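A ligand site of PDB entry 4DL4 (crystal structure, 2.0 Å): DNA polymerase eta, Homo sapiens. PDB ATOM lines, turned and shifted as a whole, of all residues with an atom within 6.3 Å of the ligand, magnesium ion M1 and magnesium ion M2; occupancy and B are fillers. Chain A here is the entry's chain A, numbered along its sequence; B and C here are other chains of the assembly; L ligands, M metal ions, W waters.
The side-chain amino group of Lys 227 lies within salt-bridge range of the side-chain carboxylate of Glu 119, at 3.2 Å.
The side-chain hydroxyl (OH) of Tyr 55 sits close to the guanidinium group (NH1) of Arg 58 (3.2 Å).
The backbone carbonyl oxygen (O) of Ile 51 lies within hydrogen-bond range of the guanidinium group (NE) of Arg 64 (2.9 Å).
The backbone carbonyl oxygen (O) of Asp 16 sits at hydrogen-bond distance from the side-chain amino group (NZ) of Lys 234, 3.1 Å away.
The backbone NH (N) of Glu 119 lies close to the side-chain hydroxyl (OG) of Ser 116, 3.3 Å away.
O2 of DC 3 of chain C lies close to N2 of DG 9 of chain B (2.7 Å).
The backbone NH of Asp 118 sits close to the side-chain hydroxyl of Ser 116, at 3.1 Å.
NE of Arg 58 sits at hydrogen-bond distance from O of Val 53 (2.8 Å).
Merely in contact with magnesium ion M2: Lys 234.
Within 4 Å of magnesium ion M2: Asp 16, Met 17, Asp 118 and Lys 234.
The nearest printed residue that does not touch magnesium ion M2 is Cys 19 (4.3 Å).
The side-chain amino group (NZ) of Lys 234 is in salt-bridge range of an oxygen (O3) of the ligand, 3.2 Å away.
An oxygen (O4) of the ligand sits at hydrogen-bond distance from the backbone NH of Phe 20, at 3.3 Å.
A nitrogen (N4) of the ligand sits at hydrogen-bond distance from O6 of DG 2 of chain C.
The backbone NH (N) of Cys 19 lies within hydrogen-bond range of an oxygen (O3) of the ligand, at 2.9 Å.
O1 of the ligand is in salt-bridge range of NH1 of Arg 58 (3.3 Å).
The side-chain hydroxyl (OH) of Tyr 55 sits at hydrogen-bond distance from an oxygen (O3) of the ligand, at 2.6 Å.
N of Phe 21 lies within hydrogen-bond range of O11 of the ligand (3.3 Å).
O4 of the ligand is in salt-bridge range of NH2 of Arg 64, 3.8 Å away.
O7 of the ligand binds magnesium ion M2 (2.2 Å).
Magnesium ion M2 is bound by O5 of the ligand.
The side-chain carboxylate (OD2) of Asp 16 binds magnesium ion M2 (2.2 Å).
Magnesium ion M2 is bound by O of Met 17 (2.2 Å).
The side-chain carboxylate (OD2) of Asp 118 binds magnesium ion M2.
An oxygen (O2) of the ligand binds magnesium ion M2 (2.2 Å).
Magnesium ion M2 has six donor atoms within binding distance.
Magnesium ion M1 is bound by O7 of the ligand (2.1 Å), OE1 of Glu 119 (2.2 Å), OD1 of Asp 16 (2.2 Å), OD1 of Asp 118 (2.2 Å), O3' of DG 9 of chain B (2.3 Å) and water W5 (2.3 Å).
Magnesium ion M1 has six donor atoms within binding distance.
Asp 18 touches the ligand.
Ile 51 touches the ligand (O to C4, 3.5 Å).
Ala 52 touches the ligand (CB to O11, 3.6 Å).
Ile 117 touches the ligand.
Hydrophobic or aromatic side chains that line the ligand: Phe 20, Phe 21, Ala 52, Tyr 55 and Ile 117.
Water W2 bridges O12 of the ligand (2.9 Å) and N2 of DG 2 of chain C (3.2 Å).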
ATOM      1  N   ASP A  16     -20.622 -18.041  -1.064  1.00  0.00           N
ATOM      2  CA  ASP A  16     -19.705 -18.752  -1.939  1.00  0.00           C
ATOM      3  C   ASP A  16     -19.692 -18.180  -3.360  1.00  0.00           C
ATOM      4  O   ASP A  16     -20.740 -18.064  -3.987  1.00  0.00           O
ATOM      5  CB  ASP A  16     -20.094 -20.211  -1.984  1.00  0.00           C
ATOM      6  CG  ASP A  16     -19.095 -21.036  -2.733  1.00  0.00           C
ATOM      7  OD1 ASP A  16     -18.210 -21.612  -2.074  1.00  0.00           O
ATOM      8  OD2 ASP A  16     -19.190 -21.070  -3.969  1.00  0.00           O
ATOM      9  N   MET A  17     -18.503 -17.845  -3.857  1.00  0.00           N
ATOM     10  CA  MET A  17     -18.374 -17.233  -5.182  1.00  0.00           C
ATOM     11  C   MET A  17     -18.795 -18.213  -6.275  1.00  0.00           C
ATOM     12  O   MET A  17     -18.530 -19.401  -6.178  1.00  0.00           O
ATOM     13  CB  MET A  17     -16.929 -16.783  -5.427  1.00  0.00           C
ATOM     14  CG  MET A  17     -16.331 -15.963  -4.294  1.00  0.00           C
ATOM     15  SD  MET A  17     -17.351 -14.515  -3.922  1.00  0.00           S
ATOM     16  CE  MET A  17     -17.179 -13.589  -5.431  1.00  0.00           C
ATOM     17  N   ASP A  18     -19.410 -17.714  -7.344  1.00  0.00           N
ATOM     18  CA  ASP A  18     -19.838 -18.589  -8.432  1.00  0.00           C
ATOM     19  C   ASP A  18     -18.650 -18.854  -9.390  1.00  0.00           C
ATOM     20  O   ASP A  18     -18.050 -17.925  -9.895  1.00  0.00           O
ATOM     21  CB  ASP A  18     -20.997 -17.947  -9.183  1.00  0.00           C
ATOM     22  CG  ASP A  18     -22.247 -17.767  -8.305  1.00  0.00           C
ATOM     23  OD1 ASP A  18     -22.410 -18.513  -7.342  1.00  0.00           O
ATOM     24  OD2 ASP A  18     -23.052 -16.869  -8.581  1.00  0.00           O
ATOM     25  N   CYS A  19     -18.301 -20.118  -9.586  1.00  0.00           N
ATOM     26  CA  CYS A  19     -17.244 -20.468 -10.556  1.00  0.00           C
ATOM     27  C   CYS A  19     -16.030 -19.557 -10.421  1.00  0.00           C
ATOM     28  O   CYS A  19     -15.638 -18.875 -11.365  1.00  0.00           O
ATOM     29  CB  CYS A  19     -17.749 -20.550 -11.997  1.00  0.00           C
ATOM     30  SG  CYS A  19     -18.426 -19.038 -12.684  1.00  0.00           S
ATOM     31  N   PHE A  20     -15.456 -19.503  -9.218  1.00  0.00           N
ATOM     32  CA  PHE A  20     -14.625 -18.378  -8.814  1.00  0.00           C
ATOM     33  C   PHE A  20     -13.369 -18.113  -9.640  1.00  0.00           C
ATOM     34  O   PHE A  20     -13.164 -16.983 -10.053  1.00  0.00           O
ATOM     35  CB  PHE A  20     -14.208 -18.569  -7.361  1.00  0.00           C
ATOM     36  CG  PHE A  20     -13.384 -17.459  -6.816  1.00  0.00           C
ATOM     37  CD1 PHE A  20     -13.797 -16.153  -6.950  1.00  0.00           C
ATOM     38  CD2 PHE A  20     -12.181 -17.717  -6.194  1.00  0.00           C
ATOM     39  CE1 PHE A  20     -13.045 -15.121  -6.456  1.00  0.00           C
ATOM     40  CE2 PHE A  20     -11.417 -16.686  -5.694  1.00  0.00           C
ATOM     41  CZ  PHE A  20     -11.854 -15.379  -5.828  1.00  0.00           C
ATOM     42  N   PHE A  21     -12.580 -19.136  -9.937  1.00  0.00           N
ATOM     43  CA  PHE A  21     -11.381 -18.926 -10.758  1.00  0.00           C
ATOM     44  C   PHE A  21     -11.750 -18.414 -12.155  1.00  0.00           C
ATOM     45  O   PHE A  21     -11.049 -17.573 -12.717  1.00  0.00           O
ATOM     46  CB  PHE A  21     -10.524 -20.189 -10.865  1.00  0.00           C
ATOM     47  CG  PHE A  21      -9.793 -20.560  -9.600  1.00  0.00           C
ATOM     48  CD1 PHE A  21     -10.134 -19.999  -8.377  1.00  0.00           C
ATOM     49  CD2 PHE A  21      -8.757 -21.479  -9.631  1.00  0.00           C
ATOM     50  CE1 PHE A  21      -9.467 -20.362  -7.221  1.00  0.00           C
ATOM     51  CE2 PHE A  21      -8.081 -21.831  -8.475  1.00  0.00           C
ATOM     52  CZ  PHE A  21      -8.438 -21.275  -7.267  1.00  0.00           C
ATOM     53  N   VAL A  22     -12.843 -18.931 -12.721  1.00  0.00           N
ATOM     54  CA  VAL A  22     -13.329 -18.463 -14.017  1.00  0.00           C
ATOM     55  C   VAL A  22     -13.687 -16.963 -13.987  1.00  0.00           C
ATOM     56  O   VAL A  22     -13.306 -16.211 -14.883  1.00  0.00           O
ATOM     57  CB  VAL A  22     -14.542 -19.285 -14.500  1.00  0.00           C
ATOM     58  CG1 VAL A  22     -15.170 -18.653 -15.734  1.00  0.00           C
ATOM     59  CG2 VAL A  22     -14.128 -20.732 -14.782  1.00  0.00           C
ATOM     60  N   ILE A  51      -9.767 -27.076 -13.521  1.00  0.00           N
ATOM     61  CA  ILE A  51     -10.066 -26.915 -12.107  1.00  0.00           C
ATOM     62  C   ILE A  51     -11.270 -25.996 -11.816  1.00  0.00           C
ATOM     63  O   ILE A  51     -11.746 -25.949 -10.685  1.00  0.00           O
ATOM     64  CB  ILE A  51      -8.843 -26.444 -11.316  1.00  0.00           C
ATOM     65  CG1 ILE A  51      -8.354 -25.093 -11.837  1.00  0.00           C
ATOM     66  CG2 ILE A  51      -7.725 -27.490 -11.405  1.00  0.00           C
ATOM     67  CD1 ILE A  51      -7.138 -24.570 -11.096  1.00  0.00           C
ATOM     68  N   ALA A  52     -11.741 -25.278 -12.831  1.00  0.00           N
ATOM     69  CA  ALA A  52     -12.953 -24.475 -12.680  1.00  0.00           C
ATOM     70  C   ALA A  52     -13.684 -24.319 -14.013  1.00  0.00           C
ATOM     71  O   ALA A  52     -13.057 -24.217 -15.067  1.00  0.00           O
ATOM     72  CB  ALA A  52     -12.621 -23.113 -12.084  1.00  0.00           C
ATOM     73  N   VAL A  53     -15.019 -24.273 -13.952  1.00  0.00           N
ATOM     74  CA  VAL A  53     -15.843 -24.335 -15.146  1.00  0.00           C
ATOM     75  C   VAL A  53     -16.995 -23.334 -15.073  1.00  0.00           C
ATOM     76  O   VAL A  53     -17.726 -23.297 -14.082  1.00  0.00           O
ATOM     77  CB  VAL A  53     -16.431 -25.750 -15.337  1.00  0.00           C
ATOM     78  CG1 VAL A  53     -17.185 -25.846 -16.655  1.00  0.00           C
ATOM     79  CG2 VAL A  53     -15.338 -26.799 -15.258  1.00  0.00           C
ATOM     80  N   TYR A  55     -20.652 -21.623 -15.867  1.00  0.00           N
ATOM     81  CA  TYR A  55     -21.974 -22.216 -15.968  1.00  0.00           C
ATOM     82  C   TYR A  55     -22.390 -22.476 -17.416  1.00  0.00           C
ATOM     83  O   TYR A  55     -23.062 -23.471 -17.693  1.00  0.00           O
ATOM     84  CB  TYR A  55     -22.999 -21.390 -15.192  1.00  0.00           C
ATOM     85  CG  TYR A  55     -22.911 -21.654 -13.719  1.00  0.00           C
ATOM     86  CD1 TYR A  55     -21.945 -21.025 -12.935  1.00  0.00           C
ATOM     87  CD2 TYR A  55     -23.741 -22.575 -13.106  1.00  0.00           C
ATOM     88  CE1 TYR A  55     -21.839 -21.291 -11.582  1.00  0.00           C
ATOM     89  CE2 TYR A  55     -23.648 -22.841 -11.746  1.00  0.00           C
ATOM     90  CZ  TYR A  55     -22.696 -22.199 -10.991  1.00  0.00           C
ATOM     91  OH  TYR A  55     -22.598 -22.459  -9.638  1.00  0.00           O
ATOM     92  N   ARG A  58     -20.791 -25.653 -18.180  1.00  0.00           N
ATOM     93  CA  ARG A  58     -21.408 -26.747 -17.441  1.00  0.00           C
ATOM     94  C   ARG A  58     -22.631 -27.309 -18.161  1.00  0.00           C
ATOM     95  O   ARG A  58     -22.931 -28.500 -18.050  1.00  0.00           O
ATOM     96  CB  ARG A  58     -21.786 -26.298 -16.027  1.00  0.00           C
ATOM     97  CG  ARG A  58     -20.585 -25.883 -15.194  1.00  0.00           C
ATOM     98  CD  ARG A  58     -20.976 -25.532 -13.766  1.00  0.00           C
ATOM     99  NE  ARG A  58     -19.873 -24.865 -13.074  1.00  0.00           N
ATOM    100  CZ  ARG A  58     -19.875 -24.547 -11.782  1.00  0.00           C
ATOM    101  NH1 ARG A  58     -20.920 -24.842 -11.023  1.00  0.00           N
ATOM    102  NH2 ARG A  58     -18.820 -23.937 -11.255  1.00  0.00           N
ATOM    103  N   ARG A  64     -15.211 -30.452 -13.470  1.00  0.00           N
ATOM    104  CA  ARG A  64     -13.884 -30.266 -12.875  1.00  0.00           C
ATOM    105  C   ARG A  64     -12.902 -31.426 -13.062  1.00  0.00           C
ATOM    106  O   ARG A  64     -11.694 -31.210 -13.090  1.00  0.00           O
ATOM    107  CB  ARG A  64     -14.007 -29.958 -11.370  1.00  0.00           C
ATOM    108  CG  ARG A  64     -12.748 -30.327 -10.595  1.00  0.00           C
ATOM    109  CD  ARG A  64     -12.668 -29.644  -9.246  1.00  0.00           C
ATOM    110  NE  ARG A  64     -12.903 -28.210  -9.359  1.00  0.00           N
ATOM    111  CZ  ARG A  64     -14.012 -27.613  -8.953  1.00  0.00           C
ATOM    112  NH1 ARG A  64     -14.979 -28.324  -8.398  1.00  0.00           N
ATOM    113  NH2 ARG A  64     -14.161 -26.299  -9.102  1.00  0.00           N
ATOM    114  N   LEU A  92      -1.000 -20.065  -7.649  1.00  0.00           N
ATOM    115  CA  LEU A  92      -2.382 -19.617  -7.446  1.00  0.00           C
ATOM    116  C   LEU A  92      -2.483 -18.208  -6.893  1.00  0.00           C
ATOM    117  O   LEU A  92      -3.543 -17.815  -6.397  1.00  0.00           O
ATOM    118  CB  LEU A  92      -3.108 -20.593  -6.515  1.00  0.00           C
ATOM    119  CG  LEU A  92      -3.086 -22.061  -6.937  1.00  0.00           C
ATOM    120  CD1 LEU A  92      -3.748 -22.929  -5.863  1.00  0.00           C
ATOM    121  CD2 LEU A  92      -3.762 -22.254  -8.278  1.00  0.00           C
ATOM    122  N   SER A 116     -12.764 -21.336   2.808  1.00  0.00           N
ATOM    123  CA  SER A 116     -11.951 -21.731   1.663  1.00  0.00           C
ATOM    124  C   SER A 116     -11.530 -20.483   0.913  1.00  0.00           C
ATOM    125  O   SER A 116     -11.857 -19.368   1.309  1.00  0.00           O
ATOM    126  CB  SER A 116     -12.725 -22.661   0.728  1.00  0.00           C
ATOM    127  OG  SER A 116     -13.600 -21.926  -0.130  1.00  0.00           O
ATOM    128  N   ILE A 117     -10.810 -20.670  -0.190  1.00  0.00           N
ATOM    129  CA  ILE A 117     -10.392 -19.526  -0.982  1.00  0.00           C
ATOM    130  C   ILE A 117     -11.582 -18.712  -1.502  1.00  0.00           C
ATOM    131  O   ILE A 117     -11.468 -17.506  -1.715  1.00  0.00           O
ATOM    132  CB  ILE A 117      -9.505 -19.960  -2.165  1.00  0.00           C
ATOM    133  CG1 ILE A 117      -8.762 -18.746  -2.750  1.00  0.00           C
ATOM    134  CG2 ILE A 117     -10.320 -20.693  -3.217  1.00  0.00           C
ATOM    135  CD1 ILE A 117      -7.631 -19.128  -3.696  1.00  0.00           C
ATOM    136  N   ASP A 118     -12.742 -19.349  -1.687  1.00  0.00           N
ATOM    137  CA  ASP A 118     -13.851 -18.634  -2.302  1.00  0.00           C
ATOM    138  C   ASP A 118     -15.127 -18.603  -1.459  1.00  0.00           C
ATOM    139  O   ASP A 118     -16.201 -18.252  -1.962  1.00  0.00           O
ATOM    140  CB  ASP A 118     -14.149 -19.207  -3.684  1.00  0.00           C
ATOM    141  CG  ASP A 118     -15.242 -20.227  -3.649  1.00  0.00           C
ATOM    142  OD1 ASP A 118     -15.192 -21.114  -2.766  1.00  0.00           O
ATOM    143  OD2 ASP A 118     -16.150 -20.143  -4.481  1.00  0.00           O
ATOM    144  N   GLU A 119     -15.022 -18.939  -0.176  1.00  0.00           N
ATOM    145  CA  GLU A 119     -16.195 -18.873   0.679  1.00  0.00           C
ATOM    146  C   GLU A 119     -15.903 -18.559   2.141  1.00  0.00           C
ATOM    147  O   GLU A 119     -14.798 -18.790   2.644  1.00  0.00           O
ATOM    148  CB  GLU A 119     -17.022 -20.164   0.567  1.00  0.00           C
ATOM    149  CG  GLU A 119     -16.356 -21.358   1.179  1.00  0.00           C
ATOM    150  CD  GLU A 119     -16.856 -22.660   0.574  1.00  0.00           C
ATOM    151  OE1 GLU A 119     -16.313 -23.051  -0.478  1.00  0.00           O
ATOM    152  OE2 GLU A 119     -17.778 -23.280   1.144  1.00  0.00           O
ATOM    153  N   LYS A 227     -24.523 -23.753   4.512  1.00  0.00           N
ATOM    154  CA  LYS A 227     -23.804 -24.299   3.371  1.00  0.00           C
ATOM    155  C   LYS A 227     -24.720 -25.072   2.421  1.00  0.00           C
ATOM    156  O   LYS A 227     -24.622 -24.925   1.199  1.00  0.00           O
ATOM    157  CB  LYS A 227     -22.639 -25.199   3.807  1.00  0.00           C
ATOM    158  CG  LYS A 227     -22.024 -25.942   2.641  1.00  0.00           C
ATOM    159  CD  LYS A 227     -20.550 -26.213   2.844  1.00  0.00           C
ATOM    160  CE  LYS A 227     -19.909 -26.629   1.521  1.00  0.00           C
ATOM    161  NZ  LYS A 227     -19.978 -25.535   0.501  1.00  0.00           N
ATOM    162  N   LYS A 234     -27.744 -21.804  -6.699  1.00  0.00           N
ATOM    163  CA  LYS A 234     -26.632 -21.264  -7.478  1.00  0.00           C
ATOM    164  C   LYS A 234     -26.981 -21.298  -8.961  1.00  0.00           C
ATOM    165  O   LYS A 234     -27.660 -22.218  -9.416  1.00  0.00           O
ATOM    166  CB  LYS A 234     -25.358 -22.091  -7.244  1.00  0.00           C
ATOM    167  CG  LYS A 234     -24.432 -21.538  -6.170  1.00  0.00           C
ATOM    168  CD  LYS A 234     -23.153 -22.382  -6.077  1.00  0.00           C
ATOM    169  CE  LYS A 234     -22.110 -21.727  -5.161  1.00  0.00           C
ATOM    170  NZ  LYS A 234     -21.469 -20.530  -5.787  1.00  0.00           N
ATOM    171  N   PRO A 235     -26.507 -20.307  -9.734  1.00  0.00           N
ATOM    172  CA  PRO A 235     -25.644 -19.189  -9.314  1.00  0.00           C
ATOM    173  C   PRO A 235     -26.383 -17.868  -9.124  1.00  0.00           C
ATOM    174  O   PRO A 235     -27.535 -17.738  -9.523  1.00  0.00           O
ATOM    175  CB  PRO A 235     -24.689 -19.055 -10.508  1.00  0.00           C
ATOM    176  CG  PRO A 235     -25.557 -19.381 -11.680  1.00  0.00           C
ATOM    177  CD  PRO A 235     -26.563 -20.420 -11.194  1.00  0.00           C
ATOM    178  P    DG B   9     -16.864 -28.360   0.692  1.00  0.00           P
ATOM    179  OP1  DG B   9     -16.851 -27.996   2.133  1.00  0.00           O
ATOM    180  OP2  DG B   9     -18.040 -28.018  -0.148  1.00  0.00           O
ATOM    181  O5'  DG B   9     -15.586 -27.702   0.005  1.00  0.00           O
ATOM    182  C5'  DG B   9     -15.045 -26.467   0.528  1.00  0.00           C
ATOM    183  C4'  DG B   9     -14.216 -25.758  -0.529  1.00  0.00           C
ATOM    184  O4'  DG B   9     -12.968 -26.471  -0.729  1.00  0.00           O
ATOM    185  C3'  DG B   9     -14.875 -25.658  -1.901  1.00  0.00           C
ATOM    186  O3'  DG B   9     -14.715 -24.335  -2.424  1.00  0.00           O
ATOM    187  C2'  DG B   9     -14.109 -26.655  -2.759  1.00  0.00           C
ATOM    188  C1'  DG B   9     -12.737 -26.651  -2.117  1.00  0.00           C
ATOM    189  N9   DG B   9     -11.990 -27.896  -2.286  1.00  0.00           N
ATOM    190  C8   DG B   9     -12.466 -29.175  -2.119  1.00  0.00           C
ATOM    191  N7   DG B   9     -11.563 -30.083  -2.348  1.00  0.00           N
ATOM    192  C5   DG B   9     -10.426 -29.368  -2.682  1.00  0.00           C
ATOM    193  C6   DG B   9      -9.132 -29.824  -3.038  1.00  0.00           C
ATOM    194  O6   DG B   9      -8.712 -30.976  -3.125  1.00  0.00           O
ATOM    195  N1   DG B   9      -8.274 -28.764  -3.304  1.00  0.00           N
ATOM    196  C2   DG B   9      -8.625 -27.431  -3.244  1.00  0.00           C
ATOM    197  N2   DG B   9      -7.653 -26.551  -3.545  1.00  0.00           N
ATOM    198  N3   DG B   9      -9.826 -27.004  -2.919  1.00  0.00           N
ATOM    199  C4   DG B   9     -10.673 -28.018  -2.652  1.00  0.00           C
ATOM    200  P    DG C   1      -5.831 -40.263  -9.133  1.00  0.00           P
ATOM    201  OP1  DG C   1      -5.740 -39.219  -8.085  1.00  0.00           O
ATOM    202  OP2  DG C   1      -7.113 -40.935  -9.444  1.00  0.00           O
ATOM    203  O5'  DG C   1      -5.304 -39.702 -10.543  1.00  0.00           O
ATOM    204  C5'  DG C   1      -4.314 -38.670 -10.626  1.00  0.00           C
ATOM    205  C4'  DG C   1      -4.568 -37.828 -11.901  1.00  0.00           C
ATOM    206  O4'  DG C   1      -5.983 -37.543 -12.024  1.00  0.00           O
ATOM    207  C3'  DG C   1      -3.992 -36.448 -11.760  1.00  0.00           C
ATOM    208  O3'  DG C   1      -2.620 -36.353 -12.076  1.00  0.00           O
ATOM    209  C2'  DG C   1      -4.821 -35.688 -12.843  1.00  0.00           C
ATOM    210  C1'  DG C   1      -6.215 -36.251 -12.594  1.00  0.00           C
ATOM    211  N9   DG C   1      -6.953 -35.450 -11.613  1.00  0.00           N
ATOM    212  C8   DG C   1      -6.948 -35.700 -10.272  1.00  0.00           C
ATOM    213  N7   DG C   1      -7.736 -34.841  -9.612  1.00  0.00           N
ATOM    214  C5   DG C   1      -8.145 -33.913 -10.563  1.00  0.00           C
ATOM    215  C6   DG C   1      -8.984 -32.784 -10.390  1.00  0.00           C
ATOM    216  O6   DG C   1      -9.425 -32.375  -9.312  1.00  0.00           O
ATOM    217  N1   DG C   1      -9.245 -32.137 -11.592  1.00  0.00           N
ATOM    218  C2   DG C   1      -8.753 -32.556 -12.802  1.00  0.00           C
ATOM    219  N2   DG C   1      -9.071 -31.848 -13.937  1.00  0.00           N
ATOM    220  N3   DG C   1      -7.987 -33.646 -12.937  1.00  0.00           N
ATOM    221  C4   DG C   1      -7.715 -34.282 -11.791  1.00  0.00           C
ATOM    222  P    DG C   2      -1.627 -35.625 -11.065  1.00  0.00           P
ATOM    223  OP1  DG C   2      -0.250 -35.538 -11.585  1.00  0.00           O
ATOM    224  OP2  DG C   2      -1.845 -36.302  -9.737  1.00  0.00           O
ATOM    225  O5'  DG C   2      -2.323 -34.186 -10.881  1.00  0.00           O
ATOM    226  C5'  DG C   2      -2.029 -33.087 -11.693  1.00  0.00           C
ATOM    227  C4'  DG C   2      -2.086 -31.793 -10.867  1.00  0.00           C
ATOM    228  O4'  DG C   2      -3.431 -31.507 -10.420  1.00  0.00           O
ATOM    229  C3'  DG C   2      -1.241 -31.876  -9.600  1.00  0.00           C
ATOM    230  O3'  DG C   2      -0.664 -30.570  -9.387  1.00  0.00           O
ATOM    231  C2'  DG C   2      -2.252 -32.251  -8.534  1.00  0.00           C
ATOM    232  C1'  DG C   2      -3.418 -31.340  -9.019  1.00  0.00           C
ATOM    233  N9   DG C   2      -4.706 -31.698  -8.463  1.00  0.00           N
ATOM    234  C8   DG C   2      -5.211 -32.929  -8.219  1.00  0.00           C
ATOM    235  N7   DG C   2      -6.403 -32.847  -7.713  1.00  0.00           N
ATOM    236  C5   DG C   2      -6.728 -31.527  -7.630  1.00  0.00           C
ATOM    237  C6   DG C   2      -7.903 -30.880  -7.157  1.00  0.00           C
ATOM    238  O6   DG C   2      -8.943 -31.386  -6.721  1.00  0.00           O
ATOM    239  N1   DG C   2      -7.805 -29.475  -7.252  1.00  0.00           N
ATOM    240  C2   DG C   2      -6.669 -28.837  -7.734  1.00  0.00           C
ATOM    241  N2   DG C   2      -6.674 -27.495  -7.791  1.00  0.00           N
ATOM    242  N3   DG C   2      -5.579 -29.444  -8.176  1.00  0.00           N
ATOM    243  C4   DG C   2      -5.681 -30.791  -8.096  1.00  0.00           C
ATOM    244  P    DC C   3       0.494 -30.227  -8.335  1.00  0.00           P
ATOM    245  OP1  DC C   3       1.492 -29.648  -9.248  1.00  0.00           O
ATOM    246  OP2  DC C   3       0.847 -31.379  -7.498  1.00  0.00           O
ATOM    247  O5'  DC C   3      -0.172 -29.084  -7.439  1.00  0.00           O
ATOM    248  C5'  DC C   3      -0.498 -27.798  -8.007  1.00  0.00           C
ATOM    249  C4'  DC C   3      -1.218 -26.941  -6.997  1.00  0.00           C
ATOM    250  O4'  DC C   3      -2.531 -27.496  -6.730  1.00  0.00           O
ATOM    251  C3'  DC C   3      -0.531 -26.829  -5.640  1.00  0.00           C
ATOM    252  O3'  DC C   3      -0.655 -25.500  -5.137  1.00  0.00           O
ATOM    253  C2'  DC C   3      -1.315 -27.785  -4.762  1.00  0.00           C
ATOM    254  C1'  DC C   3      -2.709 -27.602  -5.329  1.00  0.00           C
ATOM    255  N1   DC C   3      -3.635 -28.717  -5.065  1.00  0.00           N
ATOM    256  C2   DC C   3      -4.941 -28.416  -4.666  1.00  0.00           C
ATOM    257  O2   DC C   3      -5.281 -27.228  -4.568  1.00  0.00           O
ATOM    258  N3   DC C   3      -5.807 -29.424  -4.407  1.00  0.00           N
ATOM    259  C4   DC C   3      -5.400 -30.691  -4.522  1.00  0.00           C
ATOM    260  N4   DC C   3      -6.281 -31.652  -4.251  1.00  0.00           N
ATOM    261  C5   DC C   3      -4.072 -31.028  -4.920  1.00  0.00           C
ATOM    262  C6   DC C   3      -3.231 -30.018  -5.166  1.00  0.00           C
HETATM  263  P1  LIG L   1     -19.476 -22.872  -7.851  1.00  0.00           P
HETATM  264  O1  LIG L   1     -20.122 -24.219  -7.882  1.00  0.00           O
HETATM  265  O2  LIG L   1     -19.239 -22.550  -6.434  1.00  0.00           O
HETATM  266  O3  LIG L   1     -20.335 -21.858  -8.464  1.00  0.00           O
HETATM  267  P2  LIG L   1     -16.683 -22.878  -8.039  1.00  0.00           P
HETATM  268  O4  LIG L   1     -15.700 -22.803  -9.202  1.00  0.00           O
HETATM  269  O5  LIG L   1     -16.459 -21.670  -7.262  1.00  0.00           O
HETATM  270  O6  LIG L   1     -18.125 -22.936  -8.669  1.00  0.00           O
HETATM  271  P3  LIG L   1     -15.903 -24.225  -5.557  1.00  0.00           P
HETATM  272  O7  LIG L   1     -16.722 -23.075  -4.775  1.00  0.00           O
HETATM  273  O8  LIG L   1     -16.242 -25.565  -4.837  1.00  0.00           O
HETATM  274  N1  LIG L   1     -16.449 -24.306  -7.169  1.00  0.00           N
HETATM  275  O9  LIG L   1     -14.348 -23.836  -5.442  1.00  0.00           O
HETATM  276  C1  LIG L   1     -13.879 -22.522  -5.674  1.00  0.00           C
HETATM  277  C2  LIG L   1     -12.625 -22.459  -6.384  1.00  0.00           C
HETATM  278  O10 LIG L   1     -11.678 -23.327  -5.726  1.00  0.00           O
HETATM  279  C3  LIG L   1     -12.828 -23.054  -7.719  1.00  0.00           C
HETATM  280  O11 LIG L   1     -13.195 -22.133  -8.618  1.00  0.00           O
HETATM  281  C4  LIG L   1     -11.530 -23.695  -8.030  1.00  0.00           C
HETATM  282  C5  LIG L   1     -10.965 -24.063  -6.703  1.00  0.00           C
HETATM  283  N2  LIG L   1     -11.045 -25.503  -6.535  1.00  0.00           N
HETATM  284  C6  LIG L   1      -9.981 -26.292  -6.821  1.00  0.00           C
HETATM  285  N3  LIG L   1     -10.045 -27.617  -6.654  1.00  0.00           N
HETATM  286  C7  LIG L   1     -11.158 -28.229  -6.192  1.00  0.00           C
HETATM  287  C8  LIG L   1     -12.255 -27.431  -5.894  1.00  0.00           C
HETATM  288  C9  LIG L   1     -12.183 -26.049  -6.069  1.00  0.00           C
HETATM  289  O12 LIG L   1      -8.997 -25.824  -7.223  1.00  0.00           O
HETATM  290  N4  LIG L   1     -11.205 -29.595  -6.031  1.00  0.00           N
HETATM  291 MG    MG M   1     -16.520 -22.924  -2.678  1.00  0.00          MG
HETATM  292 MG    MG M   2     -17.692 -21.292  -5.521  1.00  0.00          MG
HETATM  293  O   HOH W   1     -18.836 -26.444  -8.283  1.00  0.00           O
HETATM  294  O   HOH W   2      -6.526 -24.470  -6.613  1.00  0.00           O
HETATM  295  O   HOH W   3     -19.751 -24.240  -4.430  1.00  0.00           O
HETATM  296  O   HOH W   4     -15.851 -24.582 -11.335  1.00  0.00           O
HETATM  297  O   HOH W   5     -17.936 -24.754  -2.650  1.00  0.00           O
